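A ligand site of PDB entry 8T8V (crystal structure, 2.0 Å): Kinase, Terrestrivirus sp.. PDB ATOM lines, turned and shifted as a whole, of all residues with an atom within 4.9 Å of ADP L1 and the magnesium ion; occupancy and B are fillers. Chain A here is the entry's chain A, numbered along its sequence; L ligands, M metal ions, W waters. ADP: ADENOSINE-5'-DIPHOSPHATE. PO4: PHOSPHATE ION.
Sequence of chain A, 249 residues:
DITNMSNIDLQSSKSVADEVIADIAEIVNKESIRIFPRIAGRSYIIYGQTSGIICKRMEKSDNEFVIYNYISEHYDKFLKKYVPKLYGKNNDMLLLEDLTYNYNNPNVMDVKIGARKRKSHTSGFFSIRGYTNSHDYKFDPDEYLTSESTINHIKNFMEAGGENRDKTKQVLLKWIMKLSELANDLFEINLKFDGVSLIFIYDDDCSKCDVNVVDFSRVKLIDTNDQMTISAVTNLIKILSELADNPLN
The backbone carbonyl oxygen (O) of Glu 97 sits at hydrogen-bond distance from a nitrogen (N6) of ADP L1 (2.8 Å). The side-chain carboxylate (OD2) of Asp 110 sits at hydrogen-bond distance from an oxygen (O3') of ADP L1 (2.6 Å). O2B of ADP L1 is in hydrogen-bond range of N of Ser 43. The backbone NH of Ala 40 lies within hydrogen-bond range of an oxygen (O3') of ADP L1. The backbone NH (N) of Leu 99 lies within hydrogen-bond range of a nitrogen (N1) of ADP L1. The backbone NH of Arg 42 is in hydrogen-bond range of an oxygen (O2B) of ADP L1 (2.9 Å). O2A of ADP L1 is in salt-bridge range of NZ of Lys 56 (2.7 Å). An oxygen (O2') of ADP L1 lies within hydrogen-bond range of the backbone NH (N) of Ile 39 (3.1 Å). OG of Ser 43 sits at hydrogen-bond distance from O2B of ADP L1, 3.0 Å away.
The magnesium ion is bound by an oxygen (O1A) of ADP L1 (1.9 Å), water W4 (2.1 Å), water W2 (2.1 Å), an oxygen (O1B) of ADP L1 (2.2 Å), the side-chain carboxylate (OD2) of Asp 215 (2.2 Å) and an oxygen (O1) of PO4 L2 (2.2 Å). The magnesium ion has six donor atoms within binding distance.
Water W4 lies within hydrogen-bond range of OG of Ser 197 (2.6 Å), O of Gly 195 (2.7 Å) and NZ of Lys 112 (3.4 Å).
CE2 of Phe 36 touches N3 of ADP L1, 3.6 Å away. Arg 38 touches ADP L1. CA of Gly 41 touches O1B of ADP L1 (3.4 Å). Ile 45 touches ADP L1. Ile 54 touches ADP L1 (CD1 to C5, 3.4 Å). CB of Pro 84 touches N6 of ADP L1, at 3.7 Å. CA of Asp 98 touches N1 of ADP L1 (3.9 Å). Ile 199 touches ADP L1 (CD1 to C3', 3.96 Å). Val 214 touches ADP L1. Hydrophobic or aromatic side chains that line ADP L1: Phe 36, Ile 39, Ala 40, Ile 45, Ile 54, Pro 84, Leu 99, Ile 199 and Val 214. Of the 26 residues printed, 18 come within 4 Å of ADP L1. The nearest printed residue that does not touch ADP L1 is Leu 96 (4.2 Å).
One residue has an atom within 4 Å of the magnesium ion: Asp 215. The nearest printed residue that does not touch the magnesium ion is Ser 197 (4.1 Å).
OD1 of Asp 110 lies within hydrogen-bond range of OG of Ser 197, at 2.7 Å. The side-chain carboxylate of Asp 215 lies within hydrogen-bond range of the side-chain hydroxyl of Ser 217 (2.7 Å). The backbone carbonyl oxygen (O) of Ile 45 is in hydrogen-bond range of the backbone NH (N) of Phe 36, at 3.0 Å. The backbone carbonyl oxygen (O) of Ile 54 lies within hydrogen-bond range of the backbone NH (N) of Leu 96 (2.8 Å). OD1 of Asp 98 lies within hydrogen-bond range of OG1 of Thr 100. O of Gly 41 lies within hydrogen-bond range of NH2 of Arg 38, 2.9 Å away. The side-chain carboxylate (OD1) of Asp 215 lies within salt-bridge range of the side-chain amino group (NZ) of Lys 56 (3.6 Å). The guanidinium group (NE) of Arg 38 is in hydrogen-bond range of the backbone carbonyl oxygen (O) of Ser 43 (3.3 Å).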
ATOM      1  N   PHE A  36      -2.944   0.801  10.188  1.00  0.00           N
ATOM      2  CA  PHE A  36      -2.139  -0.449  10.169  1.00  0.00           C
ATOM      3  C   PHE A  36      -1.116  -0.344   9.042  1.00  0.00           C
ATOM      4  O   PHE A  36      -1.462   0.089   7.943  1.00  0.00           O
ATOM      5  CB  PHE A  36      -3.031  -1.678   9.997  1.00  0.00           C
ATOM      6  CG  PHE A  36      -2.287  -2.973  10.183  1.00  0.00           C
ATOM      7  CD1 PHE A  36      -1.976  -3.441  11.446  1.00  0.00           C
ATOM      8  CD2 PHE A  36      -1.831  -3.692   9.089  1.00  0.00           C
ATOM      9  CE1 PHE A  36      -1.259  -4.614  11.622  1.00  0.00           C
ATOM     10  CE2 PHE A  36      -1.109  -4.863   9.256  1.00  0.00           C
ATOM     11  CZ  PHE A  36      -0.834  -5.325  10.521  1.00  0.00           C
ATOM     12  N   ARG A  38      -0.059  -1.698   6.372  1.00  0.00           N
ATOM     13  CA  ARG A  38      -0.344  -2.480   5.136  1.00  0.00           C
ATOM     14  C   ARG A  38       0.909  -2.551   4.259  1.00  0.00           C
ATOM     15  O   ARG A  38       1.583  -1.525   4.080  1.00  0.00           O
ATOM     16  CB  ARG A  38      -1.450  -1.791   4.317  1.00  0.00           C
ATOM     17  CG  ARG A  38      -2.814  -2.425   4.467  1.00  0.00           C
ATOM     18  CD  ARG A  38      -3.952  -1.495   4.091  1.00  0.00           C
ATOM     19  NE  ARG A  38      -3.842  -0.927   2.749  1.00  0.00           N
ATOM     20  CZ  ARG A  38      -3.642   0.355   2.462  1.00  0.00           C
ATOM     21  NH1 ARG A  38      -3.479   1.246   3.428  1.00  0.00           N
ATOM     22  NH2 ARG A  38      -3.591   0.748   1.207  1.00  0.00           N
ATOM     23  N   ILE A  39       1.180  -3.724   3.684  1.00  0.00           N
ATOM     24  CA  ILE A  39       2.306  -3.895   2.724  1.00  0.00           C
ATOM     25  C   ILE A  39       1.760  -3.689   1.303  1.00  0.00           C
ATOM     26  O   ILE A  39       2.522  -3.222   0.442  1.00  0.00           O
ATOM     27  CB  ILE A  39       3.020  -5.246   2.974  1.00  0.00           C
ATOM     28  CG1 ILE A  39       4.521  -5.028   3.159  1.00  0.00           C
ATOM     29  CG2 ILE A  39       2.704  -6.278   1.910  1.00  0.00           C
ATOM     30  CD1 ILE A  39       4.851  -4.003   4.219  1.00  0.00           C
ATOM     31  N   ALA A  40       0.474  -3.938   1.079  1.00  0.00           N
ATOM     32  CA  ALA A  40      -0.191  -3.765  -0.232  1.00  0.00           C
ATOM     33  C   ALA A  40      -1.691  -3.525  -0.020  1.00  0.00           C
ATOM     34  O   ALA A  40      -2.120  -3.315   1.132  1.00  0.00           O
ATOM     35  CB  ALA A  40       0.049  -4.970  -1.091  1.00  0.00           C
ATOM     36  N   GLY A  41      -2.451  -3.546  -1.113  1.00  0.00           N
ATOM     37  CA  GLY A  41      -3.920  -3.423  -1.081  1.00  0.00           C
ATOM     38  C   GLY A  41      -4.342  -1.972  -1.044  1.00  0.00           C
ATOM     39  O   GLY A  41      -3.467  -1.091  -1.094  1.00  0.00           O
ATOM     40  N   ARG A  42      -5.646  -1.750  -0.953  1.00  0.00           N
ATOM     41  CA  ARG A  42      -6.284  -0.424  -1.136  1.00  0.00           C
ATOM     42  C   ARG A  42      -7.243  -0.085   0.011  1.00  0.00           C
ATOM     43  O   ARG A  42      -7.567   1.109   0.168  1.00  0.00           O
ATOM     44  CB  ARG A  42      -7.068  -0.447  -2.452  1.00  0.00           C
ATOM     45  CG  ARG A  42      -6.690   0.712  -3.349  1.00  0.00           C
ATOM     46  CD  ARG A  42      -7.345   2.014  -2.916  1.00  0.00           C
ATOM     47  NE  ARG A  42      -7.183   2.935  -4.037  1.00  0.00           N
ATOM     48  CZ  ARG A  42      -7.777   2.796  -5.224  1.00  0.00           C
ATOM     49  NH1 ARG A  42      -8.604   1.789  -5.455  1.00  0.00           N
ATOM     50  NH2 ARG A  42      -7.540   3.676  -6.185  1.00  0.00           N
ATOM     51  N   SER A  43      -7.690  -1.098   0.742  1.00  0.00           N
ATOM     52  CA  SER A  43      -8.749  -0.985   1.780  1.00  0.00           C
ATOM     53  C   SER A  43      -8.228  -0.213   2.983  1.00  0.00           C
ATOM     54  O   SER A  43      -7.013  -0.266   3.255  1.00  0.00           O
ATOM     55  CB  SER A  43      -9.250  -2.341   2.181  1.00  0.00           C
ATOM     56  OG  SER A  43      -9.860  -3.000   1.083  1.00  0.00           O
ATOM     57  N   ILE A  45      -7.498  -0.116   6.621  1.00  0.00           N
ATOM     58  CA  ILE A  45      -7.139  -1.112   7.670  1.00  0.00           C
ATOM     59  C   ILE A  45      -6.431  -0.401   8.820  1.00  0.00           C
ATOM     60  O   ILE A  45      -5.385   0.254   8.592  1.00  0.00           O
ATOM     61  CB  ILE A  45      -6.305  -2.278   7.107  1.00  0.00           C
ATOM     62  CG1 ILE A  45      -7.016  -2.987   5.943  1.00  0.00           C
ATOM     63  CG2 ILE A  45      -5.942  -3.255   8.225  1.00  0.00           C
ATOM     64  CD1 ILE A  45      -6.224  -4.105   5.318  1.00  0.00           C
ATOM     65  N   ILE A  54      -6.896  -6.599  13.878  1.00  0.00           N
ATOM     66  CA  ILE A  54      -6.984  -5.501  12.872  1.00  0.00           C
ATOM     67  C   ILE A  54      -8.429  -5.421  12.384  1.00  0.00           C
ATOM     68  O   ILE A  54      -9.127  -6.453  12.413  1.00  0.00           O
ATOM     69  CB  ILE A  54      -5.978  -5.678  11.710  1.00  0.00           C
ATOM     70  CG1 ILE A  54      -6.253  -6.922  10.874  1.00  0.00           C
ATOM     71  CG2 ILE A  54      -4.551  -5.666  12.246  1.00  0.00           C
ATOM     72  CD1 ILE A  54      -5.647  -6.875   9.488  1.00  0.00           C
ATOM     73  N   LYS A  56     -10.653  -4.297   9.079  1.00  0.00           N
ATOM     74  CA  LYS A  56     -10.590  -4.080   7.617  1.00  0.00           C
ATOM     75  C   LYS A  56     -11.978  -3.628   7.140  1.00  0.00           C
ATOM     76  O   LYS A  56     -12.936  -4.381   7.339  1.00  0.00           O
ATOM     77  CB  LYS A  56     -10.155  -5.358   6.877  1.00  0.00           C
ATOM     78  CG  LYS A  56     -10.163  -5.239   5.356  1.00  0.00           C
ATOM     79  CD  LYS A  56      -9.774  -6.502   4.616  1.00  0.00           C
ATOM     80  CE  LYS A  56     -10.028  -6.395   3.127  1.00  0.00           C
ATOM     81  NZ  LYS A  56      -9.639  -7.630   2.405  1.00  0.00           N
ATOM     82  N   GLU A  64     -16.950 -10.290   1.057  1.00  0.00           N
ATOM     83  CA  GLU A  64     -15.887 -10.914   1.889  1.00  0.00           C
ATOM     84  C   GLU A  64     -16.544 -11.591   3.118  1.00  0.00           C
ATOM     85  O   GLU A  64     -16.181 -12.740   3.400  1.00  0.00           O
ATOM     86  CB  GLU A  64     -14.811  -9.904   2.306  1.00  0.00           C
ATOM     87  CG  GLU A  64     -13.638 -10.556   3.020  1.00  0.00           C
ATOM     88  CD  GLU A  64     -12.301  -9.844   2.933  1.00  0.00           C
ATOM     89  OE1 GLU A  64     -12.315  -8.607   2.813  1.00  0.00           O
ATOM     90  OE2 GLU A  64     -11.257 -10.539   2.979  1.00  0.00           O
ATOM     91  N   PRO A  84      -6.744 -16.184   8.533  1.00  0.00           N
ATOM     92  CA  PRO A  84      -6.823 -15.490   9.816  1.00  0.00           C
ATOM     93  C   PRO A  84      -8.232 -15.657  10.397  1.00  0.00           C
ATOM     94  O   PRO A  84      -9.192 -15.648   9.633  1.00  0.00           O
ATOM     95  CB  PRO A  84      -6.529 -14.016   9.481  1.00  0.00           C
ATOM     96  CG  PRO A  84      -6.727 -13.911   7.979  1.00  0.00           C
ATOM     97  CD  PRO A  84      -6.357 -15.273   7.432  1.00  0.00           C
ATOM     98  N   LEU A  96     -10.396  -8.982  12.359  1.00  0.00           N
ATOM     99  CA  LEU A  96      -9.548 -10.119  11.923  1.00  0.00           C
ATOM    100  C   LEU A  96      -8.372 -10.285  12.884  1.00  0.00           C
ATOM    101  O   LEU A  96      -7.911  -9.280  13.463  1.00  0.00           O
ATOM    102  CB  LEU A  96      -9.028  -9.862  10.510  1.00  0.00           C
ATOM    103  CG  LEU A  96     -10.092  -9.863   9.409  1.00  0.00           C
ATOM    104  CD1 LEU A  96      -9.470  -9.514   8.060  1.00  0.00           C
ATOM    105  CD2 LEU A  96     -10.781 -11.210   9.326  1.00  0.00           C
ATOM    106  N   GLU A  97      -7.916 -11.530  13.019  1.00  0.00           N
ATOM    107  CA  GLU A  97      -6.623 -11.876  13.644  1.00  0.00           C
ATOM    108  C   GLU A  97      -5.499 -11.077  12.967  1.00  0.00           C
ATOM    109  O   GLU A  97      -5.403 -11.132  11.725  1.00  0.00           O
ATOM    110  CB  GLU A  97      -6.412 -13.386  13.528  1.00  0.00           C
ATOM    111  CG  GLU A  97      -5.054 -13.849  13.995  1.00  0.00           C
ATOM    112  CD  GLU A  97      -4.797 -15.317  13.677  1.00  0.00           C
ATOM    113  OE1 GLU A  97      -5.689 -15.969  13.092  1.00  0.00           O
ATOM    114  OE2 GLU A  97      -3.684 -15.792  14.007  1.00  0.00           O
ATOM    115  N   ASP A  98      -4.699 -10.360  13.752  1.00  0.00           N
ATOM    116  CA  ASP A  98      -3.485  -9.642  13.283  1.00  0.00           C
ATOM    117  C   ASP A  98      -2.360 -10.664  13.104  1.00  0.00           C
ATOM    118  O   ASP A  98      -1.816 -11.132  14.115  1.00  0.00           O
ATOM    119  CB  ASP A  98      -3.064  -8.527  14.241  1.00  0.00           C
ATOM    120  CG  ASP A  98      -1.762  -7.846  13.857  1.00  0.00           C
ATOM    121  OD1 ASP A  98      -1.196  -8.213  12.802  1.00  0.00           O
ATOM    122  OD2 ASP A  98      -1.321  -6.957  14.612  1.00  0.00           O
ATOM    123  N   LEU A  99      -2.027 -11.000  11.857  1.00  0.00           N
ATOM    124  CA  LEU A  99      -1.049 -12.086  11.554  1.00  0.00           C
ATOM    125  C   LEU A  99       0.376 -11.650  11.953  1.00  0.00           C
ATOM    126  O   LEU A  99       1.234 -12.533  12.026  1.00  0.00           O
ATOM    127  CB  LEU A  99      -1.143 -12.433  10.066  1.00  0.00           C
ATOM    128  CG  LEU A  99      -2.452 -13.092   9.611  1.00  0.00           C
ATOM    129  CD1 LEU A  99      -2.466 -13.220   8.096  1.00  0.00           C
ATOM    130  CD2 LEU A  99      -2.638 -14.460  10.262  1.00  0.00           C
ATOM    131  N   THR A 100       0.615 -10.365  12.217  1.00  0.00           N
ATOM    132  CA  THR A 100       1.960  -9.851  12.596  1.00  0.00           C
ATOM    133  C   THR A 100       2.099  -9.772  14.118  1.00  0.00           C
ATOM    134  O   THR A 100       3.210  -9.443  14.579  1.00  0.00           O
ATOM    135  CB  THR A 100       2.232  -8.480  11.977  1.00  0.00           C
ATOM    136  OG1 THR A 100       1.321  -7.537  12.543  1.00  0.00           O
ATOM    137  CG2 THR A 100       2.098  -8.479  10.466  1.00  0.00           C
ATOM    138  N   VAL A 108       6.939  -8.982   5.904  1.00  0.00           N
ATOM    139  CA  VAL A 108       5.658  -9.399   5.262  1.00  0.00           C
ATOM    140  C   VAL A 108       5.781  -9.276   3.741  1.00  0.00           C
ATOM    141  O   VAL A 108       6.316  -8.261   3.262  1.00  0.00           O
ATOM    142  CB  VAL A 108       4.479  -8.555   5.763  1.00  0.00           C
ATOM    143  CG1 VAL A 108       3.159  -9.051   5.197  1.00  0.00           C
ATOM    144  CG2 VAL A 108       4.435  -8.507   7.293  1.00  0.00           C
ATOM    145  N   ASP A 110       3.079  -9.902   0.276  1.00  0.00           N
ATOM    146  CA  ASP A 110       1.712 -10.163  -0.210  1.00  0.00           C
ATOM    147  C   ASP A 110       1.852 -10.703  -1.622  1.00  0.00           C
ATOM    148  O   ASP A 110       2.357  -9.949  -2.467  1.00  0.00           O
ATOM    149  CB  ASP A 110       0.887  -8.879  -0.160  1.00  0.00           C
ATOM    150  CG  ASP A 110      -0.523  -9.021  -0.706  1.00  0.00           C
ATOM    151  OD1 ASP A 110      -0.707  -9.771  -1.673  1.00  0.00           O
ATOM    152  OD2 ASP A 110      -1.418  -8.351  -0.151  1.00  0.00           O
ATOM    153  N   LYS A 112      -0.355 -12.208  -4.747  1.00  0.00           N
ATOM    154  CA  LYS A 112      -1.709 -12.463  -5.310  1.00  0.00           C
ATOM    155  C   LYS A 112      -1.677 -13.778  -6.088  1.00  0.00           C
ATOM    156  O   LYS A 112      -0.937 -13.859  -7.092  1.00  0.00           O
ATOM    157  CB  LYS A 112      -2.128 -11.258  -6.150  1.00  0.00           C
ATOM    158  CG  LYS A 112      -3.310 -11.499  -7.072  1.00  0.00           C
ATOM    159  CD  LYS A 112      -4.582 -10.953  -6.561  1.00  0.00           C
ATOM    160  CE  LYS A 112      -4.648  -9.443  -6.632  1.00  0.00           C
ATOM    161  NZ  LYS A 112      -5.631  -8.923  -5.649  1.00  0.00           N
ATOM    162  N   GLY A 195      -8.688 -12.879  -6.759  1.00  0.00           N
ATOM    163  CA  GLY A 195      -8.148 -11.748  -5.987  1.00  0.00           C
ATOM    164  C   GLY A 195      -7.452 -12.150  -4.691  1.00  0.00           C
ATOM    165  O   GLY A 195      -6.939 -11.237  -4.029  1.00  0.00           O
ATOM    166  N   SER A 197      -4.771 -13.400  -1.878  1.00  0.00           N
ATOM    167  CA  SER A 197      -3.322 -13.249  -1.633  1.00  0.00           C
ATOM    168  C   SER A 197      -2.871 -14.240  -0.560  1.00  0.00           C
ATOM    169  O   SER A 197      -3.675 -14.574   0.333  1.00  0.00           O
ATOM    170  CB  SER A 197      -2.997 -11.839  -1.222  1.00  0.00           C
ATOM    171  OG  SER A 197      -2.993 -10.962  -2.358  1.00  0.00           O
ATOM    172  N   ILE A 199      -0.140 -14.186   2.424  1.00  0.00           N
ATOM    173  CA  ILE A 199       0.671 -13.278   3.289  1.00  0.00           C
ATOM    174  C   ILE A 199       1.767 -14.123   3.952  1.00  0.00           C
ATOM    175  O   ILE A 199       1.440 -14.892   4.872  1.00  0.00           O
ATOM    176  CB  ILE A 199      -0.200 -12.576   4.343  1.00  0.00           C
ATOM    177  CG1 ILE A 199      -1.418 -11.894   3.718  1.00  0.00           C
ATOM    178  CG2 ILE A 199       0.633 -11.595   5.156  1.00  0.00           C
ATOM    179  CD1 ILE A 199      -1.109 -10.999   2.551  1.00  0.00           C
ATOM    180  N   VAL A 214      -5.613 -14.543   2.461  1.00  0.00           N
ATOM    181  CA  VAL A 214      -6.469 -13.372   2.817  1.00  0.00           C
ATOM    182  C   VAL A 214      -7.147 -12.813   1.571  1.00  0.00           C
ATOM    183  O   VAL A 214      -6.723 -13.161   0.442  1.00  0.00           O
ATOM    184  CB  VAL A 214      -5.671 -12.275   3.539  1.00  0.00           C
ATOM    185  CG1 VAL A 214      -4.908 -12.817   4.746  1.00  0.00           C
ATOM    186  CG2 VAL A 214      -4.726 -11.546   2.583  1.00  0.00           C
ATOM    187  N   ASP A 215      -8.146 -11.949   1.792  1.00  0.00           N
ATOM    188  CA  ASP A 215      -8.826 -11.106   0.776  1.00  0.00           C
ATOM    189  C   ASP A 215      -9.828 -11.946  -0.012  1.00  0.00           C
ATOM    190  O   ASP A 215      -9.519 -12.356  -1.148  1.00  0.00           O
ATOM    191  CB  ASP A 215      -7.837 -10.397  -0.157  1.00  0.00           C
ATOM    192  CG  ASP A 215      -8.494  -9.261  -0.924  1.00  0.00           C
ATOM    193  OD1 ASP A 215      -9.746  -9.158  -0.879  1.00  0.00           O
ATOM    194  OD2 ASP A 215      -7.748  -8.478  -1.570  1.00  0.00           O
ATOM    195  N   SER A 217     -12.776 -10.791  -0.989  1.00  0.00           N
ATOM    196  CA  SER A 217     -13.699  -9.736  -1.474  1.00  0.00           C
ATOM    197  C   SER A 217     -14.302 -10.109  -2.836  1.00  0.00           C
ATOM    198  O   SER A 217     -15.466  -9.751  -3.071  1.00  0.00           O
ATOM    199  CB  SER A 217     -13.028  -8.379  -1.510  1.00  0.00           C
ATOM    200  OG  SER A 217     -11.887  -8.378  -2.343  1.00  0.00           O
HETATM  201  PB  ADP L   1      -7.288  -5.399   0.013  1.00  0.00           P
HETATM  202  O1B ADP L   1      -6.336  -5.876  -1.052  1.00  0.00           O
HETATM  203  O2B ADP L   1      -7.170  -3.923   0.284  1.00  0.00           O
HETATM  204  O3B ADP L   1      -8.720  -5.842  -0.246  1.00  0.00           O
HETATM  205  PA  ADP L   1      -6.133  -7.507   1.670  1.00  0.00           P
HETATM  206  O1A ADP L   1      -5.557  -8.029   0.411  1.00  0.00           O
HETATM  207  O2A ADP L   1      -7.073  -8.376   2.448  1.00  0.00           O
HETATM  208  O3A ADP L   1      -6.866  -6.112   1.395  1.00  0.00           O
HETATM  209  O5' ADP L   1      -4.942  -7.017   2.638  1.00  0.00           O
HETATM  210  C5' ADP L   1      -4.069  -5.927   2.226  1.00  0.00           C
HETATM  211  C4' ADP L   1      -2.838  -5.914   3.086  1.00  0.00           C
HETATM  212  O4' ADP L   1      -3.222  -5.826   4.479  1.00  0.00           O
HETATM  213  C3' ADP L   1      -1.937  -7.154   3.010  1.00  0.00           C
HETATM  214  O3' ADP L   1      -0.959  -6.992   1.991  1.00  0.00           O
HETATM  215  C2' ADP L   1      -1.298  -7.191   4.400  1.00  0.00           C
HETATM  216  O2' ADP L   1      -0.167  -6.346   4.470  1.00  0.00           O
HETATM  217  C1' ADP L   1      -2.406  -6.646   5.284  1.00  0.00           C
HETATM  218  N9  ADP L   1      -3.268  -7.644   5.921  1.00  0.00           N
HETATM  219  C8  ADP L   1      -4.497  -8.088   5.513  1.00  0.00           C
HETATM  220  N7  ADP L   1      -5.052  -8.953   6.322  1.00  0.00           N
HETATM  221  C5  ADP L   1      -4.145  -9.061   7.368  1.00  0.00           C
HETATM  222  C6  ADP L   1      -4.155  -9.808   8.571  1.00  0.00           C
HETATM  223  N6  ADP L   1      -5.160 -10.607   8.935  1.00  0.00           N
HETATM  224  N1  ADP L   1      -3.093  -9.674   9.400  1.00  0.00           N
HETATM  225  C2  ADP L   1      -2.098  -8.865   9.032  1.00  0.00           C
HETATM  226  N3  ADP L   1      -1.977  -8.126   7.935  1.00  0.00           N
HETATM  227  C4  ADP L   1      -3.046  -8.266   7.136  1.00  0.00           C
HETATM  228  P   PO4 L   2      -4.915  -5.996  -4.207  1.00  0.00           P
HETATM  229  O1  PO4 L   2      -5.595  -7.238  -3.637  1.00  0.00           O
HETATM  230  O2  PO4 L   2      -5.123  -5.932  -5.714  1.00  0.00           O
HETATM  231  O3  PO4 L   2      -3.413  -6.042  -3.919  1.00  0.00           O
HETATM  232  O4  PO4 L   2      -5.541  -4.741  -3.561  1.00  0.00           O
HETATM  233 MG    MG M   1      -5.623  -7.872  -1.516  1.00  0.00          MG
HETATM  234  O   HOH W   1       0.643  -6.944   6.935  1.00  0.00           O
HETATM  235  O   HOH W   2      -3.549  -7.326  -1.606  1.00  0.00           O
HETATM  236  O   HOH W   3      -7.594  -9.537   5.030  1.00  0.00           O
HETATM  237  O   HOH W   4      -5.345  -9.772  -2.356  1.00  0.00           O
